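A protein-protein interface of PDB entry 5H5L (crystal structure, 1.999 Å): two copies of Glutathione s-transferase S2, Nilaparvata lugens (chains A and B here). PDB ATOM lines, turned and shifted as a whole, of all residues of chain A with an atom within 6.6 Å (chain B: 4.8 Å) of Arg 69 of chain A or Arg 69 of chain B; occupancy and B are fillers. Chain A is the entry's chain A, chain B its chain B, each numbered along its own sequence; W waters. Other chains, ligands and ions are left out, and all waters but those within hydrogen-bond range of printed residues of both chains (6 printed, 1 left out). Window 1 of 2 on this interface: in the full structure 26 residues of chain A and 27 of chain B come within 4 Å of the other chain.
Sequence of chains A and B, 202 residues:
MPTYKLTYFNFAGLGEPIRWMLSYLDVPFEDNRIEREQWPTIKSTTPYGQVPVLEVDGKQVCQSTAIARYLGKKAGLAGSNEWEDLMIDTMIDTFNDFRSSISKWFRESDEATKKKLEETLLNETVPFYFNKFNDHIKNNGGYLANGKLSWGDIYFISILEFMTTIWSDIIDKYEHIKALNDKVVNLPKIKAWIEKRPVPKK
The guanidinium group (NE) of Arg 69 of chain A lies within salt-bridge range of the side-chain carboxylate (OD1) of Asp 89 of chain A (2.9 Å). OD1 of Asp 89 of chain B lies within salt-bridge range of NE of Arg 69 of chain B (2.8 Å).
Ala 66 of chain A touches Asp 89 of chain B, and with the chains exchanged Asp 89 of chain A touches Ala 66 of chain B. Arg 69 of chain B touches its own counterpart, Arg 69 of chain A. Arg 69 of chain A touches Asp 89 of chain B, and with the chains exchanged Asp 89 of chain A touches Arg 69 of chain B.
Arg 69 of chain A touches just these residues of chain B: Arg 69 (3.4 Å) and Asp 89 (3.0 Å). Arg 69 of chain B touches two residues of chain A. Printed residues of chain A within 4 Å of Asp 89 of chain B: Ala 66 and Arg 69. Printed residues of chain B within 4 Å of Asp 93 of chain A: Thr 65 (3.7 Å) and Ala 66 (3.4 Å). Printed residues of chain B within 4 Å of Ala 66 of chain A: Asp 89. Printed residues of chain B within 4 Å of Thr 90 of chain A: Ala 66 (3.7 Å). Thr 65 of chain A touches none of the printed residues of chain B. The nearest printed residue of chain B that does not touch Thr 90 of chain A is Ile 67 of chain B (6.0 Å).
The side-chain carboxylate of Asp 89 of chain A lies within salt-bridge range of the guanidinium group of Arg 69 of chain B. The side-chain carboxylate (OD2) of Asp 93 of chain A is in hydrogen-bond range of the backbone NH (N) of Ala 66 of chain B, 3.4 Å away. The guanidinium group of Arg 69 of chain A is in salt-bridge range of the side-chain carboxylate of Asp 89 of chain B. The guanidinium group (NH2) of Arg 69 of chain A lies close to the guanidinium group (NH1) of Arg 69 of chain B.
Water W6 lies within hydrogen-bond range of the side-chain carboxylate (OD2) of Asp 89 of chain B (2.7 Å) and the side-chain amino group (NZ) of Lys 73 of chain A (2.9 Å). Water W5 bridges O of Ala 66 of chain B and OD2 of Asp 89 of chain A. Water W3 bridges OD2 of Asp 89 of chain B and O of Ala 66 of chain A. Water W2 lies within hydrogen-bond range of OD2 of Asp 93 of chain A (2.9 Å) and N of Thr 65 of chain B (3.0 Å). Water W1 bridges the side-chain amino group of Lys 73 of chain A (3.0 Å) and the side-chain amino group of Lys 73 of chain B (3.1 Å). Water W4 lies within hydrogen-bond range of the guanidinium group (NH2) of Arg 69 of chain A (3.1 Å), the guanidinium group (NH2) of Arg 69 of chain B (3.2 Å) and the side-chain carboxylate (OD1) of Asp 93 of chain A (3.2 Å).
Hydrophobic or aromatic side chains of chain A that line the printed part of chain B: Ala 66. Of the 11 printed residues of chain B, 5 touch a printed residue of chain A. Printed residues of chain B that touch a printed residue of chain A: Thr 65, Ala 66, Arg 69, Tyr 70 and Asp 89. Among the printed residues, 9 pairs touch across the chains. Among the printed residues, Asp or Glu carboxylates within 4 Å of a Lys or Arg side-chain nitrogen of the other chain: Arg 69 of chain A with Asp 89 of chain B and Asp 89 of chain A with Arg 69 of chain B.
Ala 66 of chain A touches Asp 89 of chain B. Glu 82 of chain A touches Tyr 70 of chain B (O to CD1, 3.5 Å). CB of Asp 89 of chain A touches CB of Ala 66 of chain B, at 3.7 Å. Thr 90 of chain A touches Ala 66 of chain B (N to CB, 3.7 Å). Thr 65 of chain B touches Asp 93 of chain A.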
ATOM      1  N   MET A  21      13.508  -4.318 -30.768  1.00  0.00           N
ATOM      2  CA  MET A  21      13.210  -3.238 -31.705  1.00  0.00           C
ATOM      3  C   MET A  21      14.402  -2.971 -32.628  1.00  0.00           C
ATOM      4  O   MET A  21      14.223  -2.777 -33.835  1.00  0.00           O
ATOM      5  CB  MET A  21      12.791  -1.982 -30.921  1.00  0.00           C
ATOM      6  CG  MET A  21      11.348  -1.986 -30.417  1.00  0.00           C
ATOM      7  SD  MET A  21      10.108  -2.325 -31.663  1.00  0.00           S
ATOM      8  CE  MET A  21      10.622  -1.200 -32.947  1.00  0.00           C
ATOM      9  N   SER A  64      13.343   2.872 -21.186  1.00  0.00           N
ATOM     10  CA  SER A  64      13.052   1.812 -22.134  1.00  0.00           C
ATOM     11  C   SER A  64      11.812   2.147 -22.969  1.00  0.00           C
ATOM     12  O   SER A  64      11.771   1.831 -24.154  1.00  0.00           O
ATOM     13  CB  SER A  64      12.871   0.472 -21.404  1.00  0.00           C
ATOM     14  OG  SER A  64      11.693   0.446 -20.597  1.00  0.00           O
ATOM     15  N   THR A  65      10.768   2.737 -22.367  1.00  0.00           N
ATOM     16  CA  THR A  65       9.563   3.005 -23.152  1.00  0.00           C
ATOM     17  C   THR A  65       9.826   4.089 -24.190  1.00  0.00           C
ATOM     18  O   THR A  65       9.430   3.961 -25.349  1.00  0.00           O
ATOM     19  CB  THR A  65       8.415   3.406 -22.226  1.00  0.00           C
ATOM     20  OG1 THR A  65       8.140   2.333 -21.315  1.00  0.00           O
ATOM     21  CG2 THR A  65       7.174   3.692 -23.020  1.00  0.00           C
ATOM     22  N   ALA A  66      10.476   5.172 -23.770  1.00  0.00           N
ATOM     23  CA  ALA A  66      10.827   6.252 -24.685  1.00  0.00           C
ATOM     24  C   ALA A  66      11.664   5.754 -25.855  1.00  0.00           C
ATOM     25  O   ALA A  66      11.430   6.143 -27.007  1.00  0.00           O
ATOM     26  CB  ALA A  66      11.569   7.340 -23.920  1.00  0.00           C
ATOM     27  N   ILE A  67      12.633   4.885 -25.582  1.00  0.00           N
ATOM     28  CA  ILE A  67      13.509   4.399 -26.637  1.00  0.00           C
ATOM     29  C   ILE A  67      12.748   3.476 -27.581  1.00  0.00           C
ATOM     30  O   ILE A  67      12.889   3.570 -28.808  1.00  0.00           O
ATOM     31  CB  ILE A  67      14.728   3.697 -26.016  1.00  0.00           C
ATOM     32  CG1 ILE A  67      15.570   4.679 -25.242  1.00  0.00           C
ATOM     33  CG2 ILE A  67      15.601   3.046 -27.099  1.00  0.00           C
ATOM     34  CD1 ILE A  67      16.465   4.012 -24.104  1.00  0.00           C
ATOM     35  N   ALA A  68      11.946   2.570 -27.025  1.00  0.00           N
ATOM     36  CA  ALA A  68      11.162   1.650 -27.829  1.00  0.00           C
ATOM     37  C   ALA A  68      10.213   2.404 -28.760  1.00  0.00           C
ATOM     38  O   ALA A  68      10.013   1.984 -29.911  1.00  0.00           O
ATOM     39  CB  ALA A  68      10.377   0.712 -26.921  1.00  0.00           C
ATOM     40  N   ARG A  69       9.567   3.469 -28.251  1.00  0.00           N
ATOM     41  CA  ARG A  69       8.693   4.300 -29.086  1.00  0.00           C
ATOM     42  C   ARG A  69       9.468   4.966 -30.214  1.00  0.00           C
ATOM     43  O   ARG A  69       9.005   4.997 -31.359  1.00  0.00           O
ATOM     44  CB  ARG A  69       7.993   5.370 -28.230  1.00  0.00           C
ATOM     45  CG  ARG A  69       7.030   6.283 -29.037  1.00  0.00           C
ATOM     46  CD  ARG A  69       6.374   7.400 -28.202  1.00  0.00           C
ATOM     47  NE  ARG A  69       5.643   6.840 -27.057  1.00  0.00           N
ATOM     48  CZ  ARG A  69       6.084   6.859 -25.804  1.00  0.00           C
ATOM     49  NH1 ARG A  69       7.246   7.432 -25.503  1.00  0.00           N
ATOM     50  NH2 ARG A  69       5.339   6.331 -24.837  1.00  0.00           N
ATOM     51  N   TYR A  70      10.645   5.503 -29.901  1.00  0.00           N
ATOM     52  CA  TYR A  70      11.511   6.124 -30.905  1.00  0.00           C
ATOM     53  C   TYR A  70      11.875   5.138 -32.000  1.00  0.00           C
ATOM     54  O   TYR A  70      11.679   5.415 -33.197  1.00  0.00           O
ATOM     55  CB  TYR A  70      12.756   6.684 -30.231  1.00  0.00           C
ATOM     56  CG  TYR A  70      13.865   7.118 -31.170  1.00  0.00           C
ATOM     57  CD1 TYR A  70      13.799   8.349 -31.820  1.00  0.00           C
ATOM     58  CD2 TYR A  70      14.999   6.334 -31.359  1.00  0.00           C
ATOM     59  CE1 TYR A  70      14.814   8.773 -32.648  1.00  0.00           C
ATOM     60  CE2 TYR A  70      16.013   6.738 -32.191  1.00  0.00           C
ATOM     61  CZ  TYR A  70      15.913   7.969 -32.844  1.00  0.00           C
ATOM     62  OH  TYR A  70      16.902   8.428 -33.677  1.00  0.00           O
ATOM     63  N   LEU A  71      12.387   3.971 -31.612  1.00  0.00           N
ATOM     64  CA  LEU A  71      12.704   2.928 -32.575  1.00  0.00           C
ATOM     65  C   LEU A  71      11.465   2.437 -33.284  1.00  0.00           C
ATOM     66  O   LEU A  71      11.522   2.107 -34.487  1.00  0.00           O
ATOM     67  CB  LEU A  71      13.437   1.758 -31.880  1.00  0.00           C
ATOM     68  CG  LEU A  71      14.740   2.159 -31.194  1.00  0.00           C
ATOM     69  CD1 LEU A  71      15.245   0.978 -30.417  1.00  0.00           C
ATOM     70  CD2 LEU A  71      15.765   2.639 -32.213  1.00  0.00           C
ATOM     71  N   GLY A  72      10.329   2.403 -32.576  1.00  0.00           N
ATOM     72  CA  GLY A  72       9.072   2.050 -33.210  1.00  0.00           C
ATOM     73  C   GLY A  72       8.715   2.985 -34.358  1.00  0.00           C
ATOM     74  O   GLY A  72       8.307   2.545 -35.437  1.00  0.00           O
ATOM     75  N   LYS A  73       8.895   4.277 -34.152  1.00  0.00           N
ATOM     76  CA  LYS A  73       8.567   5.244 -35.193  1.00  0.00           C
ATOM     77  C   LYS A  73       9.516   5.104 -36.388  1.00  0.00           C
ATOM     78  O   LYS A  73       9.073   5.053 -37.537  1.00  0.00           O
ATOM     79  CB  LYS A  73       8.597   6.648 -34.601  1.00  0.00           C
ATOM     80  CG  LYS A  73       7.409   6.873 -33.637  1.00  0.00           C
ATOM     81  CD  LYS A  73       7.450   8.153 -32.832  1.00  0.00           C
ATOM     82  CE  LYS A  73       6.113   8.347 -32.094  1.00  0.00           C
ATOM     83  NZ  LYS A  73       6.149   9.514 -31.130  1.00  0.00           N
ATOM     84  N   LYS A  74      10.811   4.949 -36.116  1.00  0.00           N
ATOM     85  CA  LYS A  74      11.820   4.662 -37.138  1.00  0.00           C
ATOM     86  C   LYS A  74      11.516   3.388 -37.914  1.00  0.00           C
ATOM     87  O   LYS A  74      11.812   3.297 -39.116  1.00  0.00           O
ATOM     88  CB  LYS A  74      13.215   4.552 -36.488  1.00  0.00           C
ATOM     89  CG  LYS A  74      13.872   5.886 -36.163  1.00  0.00           C
ATOM     90  CD  LYS A  74      14.384   6.594 -37.439  1.00  0.00           C
ATOM     91  CE  LYS A  74      15.434   7.657 -37.133  1.00  0.00           C
ATOM     92  NZ  LYS A  74      14.899   9.035 -37.280  1.00  0.00           N
ATOM     93  N   ALA A  78       4.610   2.563 -35.490  1.00  0.00           N
ATOM     94  CA  ALA A  78       3.811   3.423 -34.628  1.00  0.00           C
ATOM     95  C   ALA A  78       2.453   3.702 -35.289  1.00  0.00           C
ATOM     96  O   ALA A  78       1.979   2.914 -36.109  1.00  0.00           O
ATOM     97  CB  ALA A  78       4.610   4.672 -34.317  1.00  0.00           C
ATOM     98  N   GLU A  82      -2.112  10.757 -34.564  1.00  0.00           N
ATOM     99  CA  GLU A  82      -1.872  10.900 -33.132  1.00  0.00           C
ATOM    100  C   GLU A  82      -2.864  10.117 -32.303  1.00  0.00           C
ATOM    101  O   GLU A  82      -2.533   9.708 -31.192  1.00  0.00           O
ATOM    102  CB  GLU A  82      -1.911  12.357 -32.727  1.00  0.00           C
ATOM    103  CG  GLU A  82      -3.249  13.000 -32.996  1.00  0.00           C
ATOM    104  CD  GLU A  82      -3.154  14.249 -33.845  1.00  0.00           C
ATOM    105  OE1 GLU A  82      -2.129  14.431 -34.528  1.00  0.00           O
ATOM    106  OE2 GLU A  82      -4.129  15.030 -33.829  1.00  0.00           O
ATOM    107  N   ASP A  85      -1.386   6.739 -32.125  1.00  0.00           N
ATOM    108  CA  ASP A  85      -0.234   6.737 -31.203  1.00  0.00           C
ATOM    109  C   ASP A  85      -0.692   6.783 -29.743  1.00  0.00           C
ATOM    110  O   ASP A  85      -0.089   6.139 -28.895  1.00  0.00           O
ATOM    111  CB  ASP A  85       0.708   7.903 -31.506  1.00  0.00           C
ATOM    112  CG  ASP A  85       1.703   7.587 -32.597  1.00  0.00           C
ATOM    113  OD1 ASP A  85       2.154   6.428 -32.685  1.00  0.00           O
ATOM    114  OD2 ASP A  85       2.057   8.506 -33.356  1.00  0.00           O
ATOM    115  N   ASP A  89       0.272   4.212 -26.815  1.00  0.00           N
ATOM    116  CA  ASP A  89       0.913   4.781 -25.623  1.00  0.00           C
ATOM    117  C   ASP A  89       0.102   4.498 -24.364  1.00  0.00           C
ATOM    118  O   ASP A  89       0.660   4.238 -23.295  1.00  0.00           O
ATOM    119  CB  ASP A  89       1.082   6.299 -25.786  1.00  0.00           C
ATOM    120  CG  ASP A  89       2.143   6.697 -26.770  1.00  0.00           C
ATOM    121  OD1 ASP A  89       2.893   5.836 -27.265  1.00  0.00           O
ATOM    122  OD2 ASP A  89       2.222   7.920 -27.076  1.00  0.00           O
ATOM    123  N   THR A  90      -1.222   4.576 -24.447  1.00  0.00           N
ATOM    124  CA  THR A  90      -2.015   4.331 -23.252  1.00  0.00           C
ATOM    125  C   THR A  90      -1.871   2.880 -22.800  1.00  0.00           C
ATOM    126  O   THR A  90      -1.697   2.620 -21.609  1.00  0.00           O
ATOM    127  CB  THR A  90      -3.493   4.709 -23.464  1.00  0.00           C
ATOM    128  OG1 THR A  90      -4.160   4.715 -22.209  1.00  0.00           O
ATOM    129  CG2 THR A  90      -4.186   3.756 -24.394  1.00  0.00           C
ATOM    130  N   ILE A  92       0.662   0.829 -23.229  1.00  0.00           N
ATOM    131  CA  ILE A  92       1.973   0.578 -22.654  1.00  0.00           C
ATOM    132  C   ILE A  92       2.131   1.258 -21.301  1.00  0.00           C
ATOM    133  O   ILE A  92       2.807   0.718 -20.423  1.00  0.00           O
ATOM    134  CB  ILE A  92       3.091   1.000 -23.613  1.00  0.00           C
ATOM    135  CG1 ILE A  92       3.075   0.137 -24.876  1.00  0.00           C
ATOM    136  CG2 ILE A  92       4.475   0.915 -22.922  1.00  0.00           C
ATOM    137  CD1 ILE A  92       3.187  -1.356 -24.641  1.00  0.00           C
ATOM    138  N   ASP A  93       1.585   2.466 -21.116  1.00  0.00           N
ATOM    139  CA  ASP A  93       1.699   3.068 -19.784  1.00  0.00           C
ATOM    140  C   ASP A  93       0.920   2.255 -18.777  1.00  0.00           C
ATOM    141  O   ASP A  93       1.383   2.086 -17.655  1.00  0.00           O
ATOM    142  CB  ASP A  93       1.224   4.515 -19.748  1.00  0.00           C
ATOM    143  CG  ASP A  93       2.268   5.509 -20.285  1.00  0.00           C
ATOM    144  OD1 ASP A  93       3.443   5.132 -20.565  1.00  0.00           O
ATOM    145  OD2 ASP A  93       1.864   6.678 -20.515  1.00  0.00           O
ATOM    146  N   TRP A 151       5.102  -1.160 -31.990  1.00  0.00           N
ATOM    147  CA  TRP A 151       6.199  -1.255 -31.035  1.00  0.00           C
ATOM    148  C   TRP A 151       5.679  -1.655 -29.653  1.00  0.00           C
ATOM    149  O   TRP A 151       6.393  -2.301 -28.891  1.00  0.00           O
ATOM    150  CB  TRP A 151       6.982   0.085 -30.996  1.00  0.00           C
ATOM    151  CG  TRP A 151       6.262   1.228 -30.371  1.00  0.00           C
ATOM    152  CD1 TRP A 151       5.546   2.166 -31.007  1.00  0.00           C
ATOM    153  CD2 TRP A 151       6.185   1.536 -28.982  1.00  0.00           C
ATOM    154  NE1 TRP A 151       5.003   3.054 -30.099  1.00  0.00           N
ATOM    155  CE2 TRP A 151       5.380   2.681 -28.842  1.00  0.00           C
ATOM    156  CE3 TRP A 151       6.704   0.938 -27.834  1.00  0.00           C
ATOM    157  CZ2 TRP A 151       5.089   3.261 -27.582  1.00  0.00           C
ATOM    158  CZ3 TRP A 151       6.411   1.500 -26.593  1.00  0.00           C
ATOM    159  CH2 TRP A 151       5.608   2.637 -26.469  1.00  0.00           C
ATOM    160  N   TYR A 155       7.231  -4.456 -27.168  1.00  0.00           N
ATOM    161  CA  TYR A 155       7.584  -4.131 -25.795  1.00  0.00           C
ATOM    162  C   TYR A 155       6.878  -5.069 -24.835  1.00  0.00           C
ATOM    163  O   TYR A 155       7.506  -5.683 -23.970  1.00  0.00           O
ATOM    164  CB  TYR A 155       7.179  -2.682 -25.527  1.00  0.00           C
ATOM    165  CG  TYR A 155       7.668  -2.089 -24.232  1.00  0.00           C
ATOM    166  CD1 TYR A 155       6.966  -2.267 -23.061  1.00  0.00           C
ATOM    167  CD2 TYR A 155       8.836  -1.362 -24.184  1.00  0.00           C
ATOM    168  CE1 TYR A 155       7.427  -1.710 -21.836  1.00  0.00           C
ATOM    169  CE2 TYR A 155       9.291  -0.819 -22.998  1.00  0.00           C
ATOM    170  CZ  TYR A 155       8.582  -0.991 -21.834  1.00  0.00           C
ATOM    171  OH  TYR A 155       9.016  -0.447 -20.650  1.00  0.00           O
ATOM    172  N   THR B  65       0.446  10.620 -18.839  1.00  0.00           N
ATOM    173  CA  THR B  65       1.540  10.916 -19.764  1.00  0.00           C
ATOM    174  C   THR B  65       1.112  10.716 -21.217  1.00  0.00           C
ATOM    175  O   THR B  65       1.386  11.573 -22.068  1.00  0.00           O
ATOM    176  CB  THR B  65       2.772  10.060 -19.455  1.00  0.00           C
ATOM    177  OG1 THR B  65       3.182  10.248 -18.092  1.00  0.00           O
ATOM    178  CG2 THR B  65       3.947  10.457 -20.313  1.00  0.00           C
ATOM    179  N   ALA B  66       0.459   9.579 -21.524  1.00  0.00           N
ATOM    180  CA  ALA B  66       0.021   9.322 -22.894  1.00  0.00           C
ATOM    181  C   ALA B  66      -0.905  10.427 -23.380  1.00  0.00           C
ATOM    182  O   ALA B  66      -0.828  10.871 -24.546  1.00  0.00           O
ATOM    183  CB  ALA B  66      -0.693   7.962 -22.986  1.00  0.00           C
ATOM    184  N   ILE B  67      -1.816  10.845 -22.510  1.00  0.00           N
ATOM    185  CA  ILE B  67      -2.788  11.875 -22.885  1.00  0.00           C
ATOM    186  C   ILE B  67      -2.098  13.219 -23.060  1.00  0.00           C
ATOM    187  O   ILE B  67      -2.358  13.944 -24.025  1.00  0.00           O
ATOM    188  CB  ILE B  67      -3.893  11.950 -21.820  1.00  0.00           C
ATOM    189  CG1 ILE B  67      -4.698  10.649 -21.792  1.00  0.00           C
ATOM    190  CG2 ILE B  67      -4.775  13.202 -22.048  1.00  0.00           C
ATOM    191  CD1 ILE B  67      -5.609  10.482 -20.596  1.00  0.00           C
ATOM    192  N   ALA B  68      -1.187  13.564 -22.146  1.00  0.00           N
ATOM    193  CA  ALA B  68      -0.460  14.829 -22.269  1.00  0.00           C
ATOM    194  C   ALA B  68       0.294  14.924 -23.592  1.00  0.00           C
ATOM    195  O   ALA B  68       0.296  15.984 -24.245  1.00  0.00           O
ATOM    196  CB  ALA B  68       0.489  14.976 -21.084  1.00  0.00           C
ATOM    197  N   ARG B  69       0.938  13.818 -24.013  1.00  0.00           N
ATOM    198  CA  ARG B  69       1.679  13.793 -25.269  1.00  0.00           C
ATOM    199  C   ARG B  69       0.733  13.983 -26.449  1.00  0.00           C
ATOM    200  O   ARG B  69       1.040  14.711 -27.396  1.00  0.00           O
ATOM    201  CB  ARG B  69       2.449  12.464 -25.399  1.00  0.00           C
ATOM    202  CG  ARG B  69       3.366  12.367 -26.658  1.00  0.00           C
ATOM    203  CD  ARG B  69       4.059  10.959 -26.815  1.00  0.00           C
ATOM    204  NE  ARG B  69       4.916  10.690 -25.651  1.00  0.00           N
ATOM    205  CZ  ARG B  69       4.608   9.864 -24.665  1.00  0.00           C
ATOM    206  NH1 ARG B  69       3.467   9.168 -24.687  1.00  0.00           N
ATOM    207  NH2 ARG B  69       5.434   9.739 -23.635  1.00  0.00           N
ATOM    208  N   TYR B  70      -0.409  13.295 -26.410  1.00  0.00           N
ATOM    209  CA  TYR B  70      -1.427  13.422 -27.442  1.00  0.00           C
ATOM    210  C   TYR B  70      -1.896  14.871 -27.575  1.00  0.00           C
ATOM    211  O   TYR B  70      -1.841  15.457 -28.664  1.00  0.00           O
ATOM    212  CB  TYR B  70      -2.603  12.500 -27.088  1.00  0.00           C
ATOM    213  CG  TYR B  70      -3.855  12.691 -27.922  1.00  0.00           C
ATOM    214  CD1 TYR B  70      -3.901  12.251 -29.241  1.00  0.00           C
ATOM    215  CD2 TYR B  70      -5.000  13.285 -27.394  1.00  0.00           C
ATOM    216  CE1 TYR B  70      -5.038  12.389 -30.009  1.00  0.00           C
ATOM    217  CE2 TYR B  70      -6.146  13.432 -28.174  1.00  0.00           C
ATOM    218  CZ  TYR B  70      -6.151  12.969 -29.475  1.00  0.00           C
ATOM    219  OH  TYR B  70      -7.239  13.057 -30.287  1.00  0.00           O
ATOM    220  N   LEU B  71      -2.315  15.479 -26.463  1.00  0.00           N
ATOM    221  CA  LEU B  71      -2.670  16.903 -26.495  1.00  0.00           C
ATOM    222  C   LEU B  71      -1.487  17.783 -26.879  1.00  0.00           C
ATOM    223  O   LEU B  71      -1.649  18.774 -27.604  1.00  0.00           O
ATOM    224  CB  LEU B  71      -3.231  17.317 -25.163  1.00  0.00           C
ATOM    225  CG  LEU B  71      -4.430  16.477 -24.761  1.00  0.00           C
ATOM    226  CD1 LEU B  71      -4.841  16.823 -23.375  1.00  0.00           C
ATOM    227  CD2 LEU B  71      -5.578  16.707 -25.716  1.00  0.00           C
ATOM    228  N   GLY B  72      -0.281  17.393 -26.496  1.00  0.00           N
ATOM    229  CA  GLY B  72       0.888  18.149 -26.918  1.00  0.00           C
ATOM    230  C   GLY B  72       1.035  18.163 -28.419  1.00  0.00           C
ATOM    231  O   GLY B  72       1.373  19.199 -29.005  1.00  0.00           O
ATOM    232  N   LYS B  73       0.818  17.009 -29.062  1.00  0.00           N
ATOM    233  CA  LYS B  73       0.828  16.967 -30.522  1.00  0.00           C
ATOM    234  C   LYS B  73      -0.239  17.891 -31.076  1.00  0.00           C
ATOM    235  O   LYS B  73       0.009  18.645 -32.013  1.00  0.00           O
ATOM    236  CB  LYS B  73       0.554  15.562 -31.065  1.00  0.00           C
ATOM    237  CG  LYS B  73       1.634  14.521 -30.881  1.00  0.00           C
ATOM    238  CD  LYS B  73       2.751  14.739 -31.853  1.00  0.00           C
ATOM    239  CE  LYS B  73       3.894  13.753 -31.573  1.00  0.00           C
ATOM    240  NZ  LYS B  73       5.100  14.063 -32.412  1.00  0.00           N
ATOM    241  N   ASP B  89      10.274  12.722 -24.350  1.00  0.00           N
ATOM    242  CA  ASP B  89       9.782  11.491 -23.730  1.00  0.00           C
ATOM    243  C   ASP B  89      10.739  10.978 -22.673  1.00  0.00           C
ATOM    244  O   ASP B  89      10.303  10.565 -21.591  1.00  0.00           O
ATOM    245  CB  ASP B  89       9.572  10.399 -24.791  1.00  0.00           C
ATOM    246  CG  ASP B  89       8.395  10.668 -25.721  1.00  0.00           C
ATOM    247  OD1 ASP B  89       7.600  11.601 -25.490  1.00  0.00           O
ATOM    248  OD2 ASP B  89       8.299   9.946 -26.733  1.00  0.00           O
ATOM    249  N   TRP B 151       5.057  19.821 -24.320  1.00  0.00           N
ATOM    250  CA  TRP B 151       4.088  19.264 -23.380  1.00  0.00           C
ATOM    251  C   TRP B 151       4.803  18.739 -22.151  1.00  0.00           C
ATOM    252  O   TRP B 151       4.244  18.732 -21.053  1.00  0.00           O
ATOM    253  CB  TRP B 151       3.255  18.136 -24.051  1.00  0.00           C
ATOM    254  CG  TRP B 151       4.066  16.913 -24.372  1.00  0.00           C
ATOM    255  CD1 TRP B 151       4.723  16.647 -25.550  1.00  0.00           C
ATOM    256  CD2 TRP B 151       4.318  15.801 -23.516  1.00  0.00           C
ATOM    257  NE1 TRP B 151       5.353  15.443 -25.477  1.00  0.00           N
ATOM    258  CE2 TRP B 151       5.122  14.905 -24.236  1.00  0.00           C
ATOM    259  CE3 TRP B 151       3.949  15.478 -22.199  1.00  0.00           C
ATOM    260  CZ2 TRP B 151       5.561  13.715 -23.702  1.00  0.00           C
ATOM    261  CZ3 TRP B 151       4.387  14.299 -21.662  1.00  0.00           C
ATOM    262  CH2 TRP B 151       5.197  13.427 -22.398  1.00  0.00           C
HETATM  263  O   HOH W   1       4.765  11.078 -33.237  1.00  0.00           O
HETATM  264  O   HOH W   2       0.867   7.770 -17.979  1.00  0.00           O
HETATM  265  O   HOH W   3      10.406   8.629 -28.028  1.00  0.00           O
HETATM  266  O   HOH W   4       5.619   7.107 -21.864  1.00  0.00           O
HETATM  267  O   HOH W   5      -0.109   9.592 -26.879  1.00  0.00           O
HETATM  268  O   HOH W   6       6.840  10.939 -28.723  1.00  0.00           O
